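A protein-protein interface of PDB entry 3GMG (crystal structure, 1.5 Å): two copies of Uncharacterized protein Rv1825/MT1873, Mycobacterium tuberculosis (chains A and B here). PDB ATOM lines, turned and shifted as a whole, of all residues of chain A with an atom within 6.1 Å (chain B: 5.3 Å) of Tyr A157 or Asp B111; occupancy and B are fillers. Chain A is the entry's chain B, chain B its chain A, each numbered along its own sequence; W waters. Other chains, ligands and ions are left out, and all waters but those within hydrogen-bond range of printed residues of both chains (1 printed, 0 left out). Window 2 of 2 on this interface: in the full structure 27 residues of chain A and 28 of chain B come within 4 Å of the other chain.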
ATOM      1  N   HIS A 155      -9.047   7.481  -3.937  1.00  0.00           N
ATOM      2  CA  HIS A 155      -8.040   7.671  -4.960  1.00  0.00           C
ATOM      3  C   HIS A 155      -7.216   6.407  -5.119  1.00  0.00           C
ATOM      4  O   HIS A 155      -6.620   5.918  -4.153  1.00  0.00           O
ATOM      5  CB  HIS A 155      -7.095   8.802  -4.574  1.00  0.00           C
ATOM      6  CG  HIS A 155      -7.784  10.113  -4.415  1.00  0.00           C
ATOM      7  ND1 HIS A 155      -7.762  10.839  -3.240  1.00  0.00           N
ATOM      8  CD2 HIS A 155      -8.560  10.804  -5.280  1.00  0.00           C
ATOM      9  CE1 HIS A 155      -8.483  11.936  -3.405  1.00  0.00           C
ATOM     10  NE2 HIS A 155      -8.979  11.936  -4.630  1.00  0.00           N
ATOM     11  N   GLN A 156      -7.143   5.924  -6.351  1.00  0.00           N
ATOM     12  CA  GLN A 156      -6.295   4.800  -6.708  1.00  0.00           C
ATOM     13  C   GLN A 156      -4.913   5.203  -7.166  1.00  0.00           C
ATOM     14  O   GLN A 156      -3.991   4.382  -7.124  1.00  0.00           O
ATOM     15  CB  GLN A 156      -6.959   3.981  -7.806  1.00  0.00           C
ATOM     16  CG  GLN A 156      -8.292   3.364  -7.379  1.00  0.00           C
ATOM     17  CD  GLN A 156      -8.138   2.267  -6.328  1.00  0.00           C
ATOM     18  OE1 GLN A 156      -7.092   1.599  -6.224  1.00  0.00           O
ATOM     19  NE2 GLN A 156      -9.199   2.075  -5.527  1.00  0.00           N
ATOM     20  N   TYR A 157      -4.765   6.441  -7.636  1.00  0.00           N
ATOM     21  CA  TYR A 157      -3.494   6.870  -8.257  1.00  0.00           C
ATOM     22  C   TYR A 157      -2.869   8.066  -7.555  1.00  0.00           C
ATOM     23  O   TYR A 157      -1.648   8.095  -7.350  1.00  0.00           O
ATOM     24  CB  TYR A 157      -3.703   7.174  -9.747  1.00  0.00           C
ATOM     25  CG  TYR A 157      -4.272   5.993 -10.483  1.00  0.00           C
ATOM     26  CD1 TYR A 157      -3.464   4.944 -10.898  1.00  0.00           C
ATOM     27  CD2 TYR A 157      -5.630   5.899 -10.704  1.00  0.00           C
ATOM     28  CE1 TYR A 157      -4.017   3.841 -11.535  1.00  0.00           C
ATOM     29  CE2 TYR A 157      -6.178   4.815 -11.342  1.00  0.00           C
ATOM     30  CZ  TYR A 157      -5.378   3.800 -11.754  1.00  0.00           C
ATOM     31  OH  TYR A 157      -5.959   2.712 -12.383  1.00  0.00           O
ATOM     32  N   ALA A 158      -3.688   9.044  -7.176  1.00  0.00           N
ATOM     33  CA  ALA A 158      -3.198  10.240  -6.496  1.00  0.00           C
ATOM     34  C   ALA A 158      -2.827   9.955  -5.036  1.00  0.00           C
ATOM     35  O   ALA A 158      -3.572   9.303  -4.307  1.00  0.00           O
ATOM     36  CB  ALA A 158      -4.244  11.376  -6.563  1.00  0.00           C
ATOM     37  N   GLN A 159      -1.673  10.465  -4.625  1.00  0.00           N
ATOM     38  CA  GLN A 159      -1.201  10.412  -3.245  1.00  0.00           C
ATOM     39  C   GLN A 159      -0.776  11.796  -2.821  1.00  0.00           C
ATOM     40  O   GLN A 159      -0.380  12.609  -3.656  1.00  0.00           O
ATOM     41  CB  GLN A 159       0.049   9.555  -3.137  1.00  0.00           C
ATOM     42  CG  GLN A 159      -0.133   8.104  -3.346  1.00  0.00           C
ATOM     43  CD  GLN A 159       1.163   7.364  -3.034  1.00  0.00           C
ATOM     44  OE1 GLN A 159       1.627   7.343  -1.883  1.00  0.00           O
ATOM     45  NE2 GLN A 159       1.763   6.791  -4.053  1.00  0.00           N
ATOM     46  N   THR B  34       0.521  13.651  -6.185  1.00  0.00           N
ATOM     47  CA  THR B  34       1.465  13.002  -7.064  1.00  0.00           C
ATOM     48  C   THR B  34       1.020  11.570  -7.354  1.00  0.00           C
ATOM     49  O   THR B  34       0.312  10.937  -6.547  1.00  0.00           O
ATOM     50  CB  THR B  34       2.880  13.036  -6.439  1.00  0.00           C
ATOM     51  OG1 THR B  34       3.824  12.525  -7.369  1.00  0.00           O
ATOM     52  CG2 THR B  34       2.947  12.231  -5.153  1.00  0.00           C
ATOM     53  N   GLY B  35       1.376  11.060  -8.513  1.00  0.00           N
ATOM     54  CA  GLY B  35       1.094   9.702  -8.901  1.00  0.00           C
ATOM     55  C   GLY B  35       1.355   9.512 -10.375  1.00  0.00           C
ATOM     56  O   GLY B  35       1.798  10.454 -11.059  1.00  0.00           O
ATOM     57  N   PRO B  36       1.098   8.326 -10.916  1.00  0.00           N
ATOM     58  CA  PRO B  36       1.256   8.138 -12.346  1.00  0.00           C
ATOM     59  C   PRO B  36       0.267   8.993 -13.107  1.00  0.00           C
ATOM     60  O   PRO B  36      -0.745   9.400 -12.550  1.00  0.00           O
ATOM     61  CB  PRO B  36       0.941   6.653 -12.546  1.00  0.00           C
ATOM     62  CG  PRO B  36       0.136   6.290 -11.391  1.00  0.00           C
ATOM     63  CD  PRO B  36       0.559   7.125 -10.254  1.00  0.00           C
ATOM     64  N   ALA B  64     -11.738   9.405 -18.167  1.00  0.00           N
ATOM     65  CA  ALA B  64     -10.729   8.371 -18.075  1.00  0.00           C
ATOM     66  C   ALA B  64     -10.198   8.139 -16.659  1.00  0.00           C
ATOM     67  O   ALA B  64      -9.222   7.397 -16.484  1.00  0.00           O
ATOM     68  CB  ALA B  64      -9.545   8.729 -19.004  1.00  0.00           C
ATOM     69  N   GLY B  65     -10.787   8.809 -15.674  1.00  0.00           N
ATOM     70  CA  GLY B  65     -10.512   8.562 -14.279  1.00  0.00           C
ATOM     71  C   GLY B  65      -9.446   9.451 -13.658  1.00  0.00           C
ATOM     72  O   GLY B  65      -8.914   9.133 -12.607  1.00  0.00           O
ATOM     73  N   GLU B  67      -7.667  11.885 -11.376  1.00  0.00           N
ATOM     74  CA  GLU B  67      -7.903  12.229  -9.969  1.00  0.00           C
ATOM     75  C   GLU B  67      -7.379  13.604  -9.557  1.00  0.00           C
ATOM     76  O   GLU B  67      -7.687  14.106  -8.468  1.00  0.00           O
ATOM     77  CB  GLU B  67      -7.317  11.125  -9.071  1.00  0.00           C
ATOM     78  CG  GLU B  67      -7.996   9.788  -9.358  1.00  0.00           C
ATOM     79  CD  GLU B  67      -7.454   8.622  -8.557  1.00  0.00           C
ATOM     80  OE1 GLU B  67      -6.398   8.780  -7.919  1.00  0.00           O
ATOM     81  OE2 GLU B  67      -8.118   7.546  -8.547  1.00  0.00           O
ATOM     82  N   ILE B 109      -3.257  13.073 -13.178  1.00  0.00           N
ATOM     83  CA  ILE B 109      -2.891  11.880 -12.417  1.00  0.00           C
ATOM     84  C   ILE B 109      -3.982  10.844 -12.581  1.00  0.00           C
ATOM     85  O   ILE B 109      -5.160  11.142 -12.364  1.00  0.00           O
ATOM     86  CB  ILE B 109      -2.653  12.206 -10.946  1.00  0.00           C
ATOM     87  CG1 ILE B 109      -1.376  13.052 -10.772  1.00  0.00           C
ATOM     88  CG2 ILE B 109      -2.519  10.915 -10.105  1.00  0.00           C
ATOM     89  CD1 ILE B 109      -1.221  13.705  -9.415  1.00  0.00           C
ATOM     90  N   GLY B 110      -3.594   9.650 -12.990  1.00  0.00           N
ATOM     91  CA  GLY B 110      -4.533   8.545 -13.261  1.00  0.00           C
ATOM     92  C   GLY B 110      -3.805   7.408 -13.943  1.00  0.00           C
ATOM     93  O   GLY B 110      -2.579   7.436 -14.033  1.00  0.00           O
ATOM     94  N   ASP B 111      -4.527   6.408 -14.452  1.00  0.00           N
ATOM     95  CA  ASP B 111      -3.885   5.315 -15.190  1.00  0.00           C
ATOM     96  C   ASP B 111      -3.357   5.845 -16.529  1.00  0.00           C
ATOM     97  O   ASP B 111      -4.141   6.229 -17.403  1.00  0.00           O
ATOM     98  CB  ASP B 111      -4.848   4.146 -15.430  1.00  0.00           C
ATOM     99  CG  ASP B 111      -4.189   3.024 -16.164  1.00  0.00           C
ATOM    100  OD1 ASP B 111      -3.205   2.490 -15.614  1.00  0.00           O
ATOM    101  OD2 ASP B 111      -4.604   2.724 -17.307  1.00  0.00           O
ATOM    102  N   PRO B 112      -2.024   5.862 -16.709  1.00  0.00           N
ATOM    103  CA  PRO B 112      -1.500   6.531 -17.920  1.00  0.00           C
ATOM    104  C   PRO B 112      -2.013   5.985 -19.268  1.00  0.00           C
ATOM    105  O   PRO B 112      -2.377   6.765 -20.140  1.00  0.00           O
ATOM    106  CB  PRO B 112       0.033   6.406 -17.756  1.00  0.00           C
ATOM    107  CG  PRO B 112       0.246   6.261 -16.346  1.00  0.00           C
ATOM    108  CD  PRO B 112      -0.917   5.441 -15.836  1.00  0.00           C
ATOM    109  N   PRO B 113      -2.107   4.647 -19.437  1.00  0.00           N
ATOM    110  CA  PRO B 113      -2.661   4.172 -20.696  1.00  0.00           C
ATOM    111  C   PRO B 113      -4.143   4.564 -20.935  1.00  0.00           C
ATOM    112  O   PRO B 113      -4.537   4.799 -22.091  1.00  0.00           O
ATOM    113  CB  PRO B 113      -2.497   2.645 -20.578  1.00  0.00           C
ATOM    114  CG  PRO B 113      -1.360   2.478 -19.647  1.00  0.00           C
ATOM    115  CD  PRO B 113      -1.513   3.552 -18.645  1.00  0.00           C
ATOM    116  N   THR B 114      -4.944   4.645 -19.875  1.00  0.00           N
ATOM    117  CA  THR B 114      -6.355   5.018 -20.015  1.00  0.00           C
ATOM    118  C   THR B 114      -6.479   6.496 -20.369  1.00  0.00           C
ATOM    119  O   THR B 114      -7.264   6.865 -21.240  1.00  0.00           O
ATOM    120  CB  THR B 114      -7.154   4.738 -18.743  1.00  0.00           C
ATOM    121  OG1 THR B 114      -6.913   3.382 -18.327  1.00  0.00           O
ATOM    122  CG2 THR B 114      -8.638   4.944 -18.969  1.00  0.00           C
ATOM    123  N   LEU B 115      -5.708   7.334 -19.670  1.00  0.00           N
ATOM    124  CA  LEU B 115      -5.704   8.770 -19.978  1.00  0.00           C
ATOM    125  C   LEU B 115      -5.227   8.999 -21.399  1.00  0.00           C
ATOM    126  O   LEU B 115      -5.809   9.795 -22.108  1.00  0.00           O
ATOM    127  CB  LEU B 115      -4.794   9.520 -18.989  1.00  0.00           C
ATOM    128  CG  LEU B 115      -5.243   9.461 -17.525  1.00  0.00           C
ATOM    129  CD1 LEU B 115      -4.160   9.987 -16.575  1.00  0.00           C
ATOM    130  CD2 LEU B 115      -6.539  10.206 -17.298  1.00  0.00           C
ATOM    131  N   ALA B 116      -4.184   8.296 -21.837  1.00  0.00           N
ATOM    132  CA  ALA B 116      -3.713   8.433 -23.211  1.00  0.00           C
ATOM    133  C   ALA B 116      -4.749   7.968 -24.218  1.00  0.00           C
ATOM    134  O   ALA B 116      -4.946   8.605 -25.247  1.00  0.00           O
ATOM    135  CB  ALA B 116      -2.400   7.691 -23.410  1.00  0.00           C
HETATM  136  O   HOH W   1      -9.884  13.680  -6.850  1.00  0.00           O
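Of chain B, only Thr B34 (3.5 Å), Gly B35 (3.5 Å), Pro B36 (3.8 Å), Glu B67 (2.9 Å), Ile B109 (3.8 Å), Gly B110 (3.8 Å) and Asp B111 (3.5 Å) come within 4 Å of Tyr A157.
Printed residues of chain A within 4 Å of Thr B34: Tyr A157, Ala A158 and Gln A159.
Of the printed residues of chain A, Gly B35 touches Tyr A157.
Ala B64 touches none of the printed residues of chain A.
Asp B111 touches one residue of chain A.
The nearest printed residue of chain A that does not touch Asp B111 is Gln A156 (7.4 Å).
The nearest printed residue of chain A that does not touch Thr B34 is Gln A156 (7.8 Å).
No position is printed for both chains.
Of the 13 pairs that touch across the chains among the printed residues, none has its exchanged pair printed and touching as well.
N of Gly B110 is in hydrogen-bond range of O of Pro B36 (2.9 Å).
The backbone NH (N) of Glu B67 lies within hydrogen-bond range of the backbone carbonyl oxygen (O) of Ile B109, 2.8 Å away.
OD2 of Asp B111 sits at hydrogen-bond distance from OG1 of Thr B114 (2.6 Å).
Among the printed residues, merely in contact across the chains: His A155 with Glu B67 (3.4 Å), Tyr A157 with Thr B34 (3.5 Å), Tyr A157 with Gly B35 (3.5 Å), Tyr A157 with Pro B36 (3.8 Å), Tyr A157 with Ile B109 (3.8 Å), Tyr A157 with Gly B110 (3.8 Å), Tyr A157 with Asp B111 (3.5 Å), Ala A158 with Thr B34 (3.6 Å) and Ala A158 with Ile B109 (3.7 Å).
Of the 5 printed residues of chain A, 5 touch a printed residue of chain B.
Printed residues of chain B that touch a printed residue of chain A: Thr B34, Gly B35, Pro B36, Glu B67, Ile B109, Gly B110 and Asp B111.
Hydrophobic or aromatic side chains of chain B that line the printed part of chain A: Pro B36 and Ile B109.
Water W1 lies within hydrogen-bond range of the backbone carbonyl oxygen of Glu B67 (2.8 Å) and a ring nitrogen (NE2) of His A155 (3.0 Å).
The side-chain carboxylate (OE1) of Glu B67 lies within hydrogen-bond range of the backbone NH (N) of Tyr A157, 2.9 Å away.
OE1 of Glu B67 lies within hydrogen-bond range of N of Ala A158.
The side-chain carboxylate of Glu B67 is in hydrogen-bond range of the backbone NH of Gln A156 (2.9 Å).
The backbone carbonyl oxygen of Thr B34 is in hydrogen-bond range of the backbone NH of Gln A159, at 2.8 Å.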
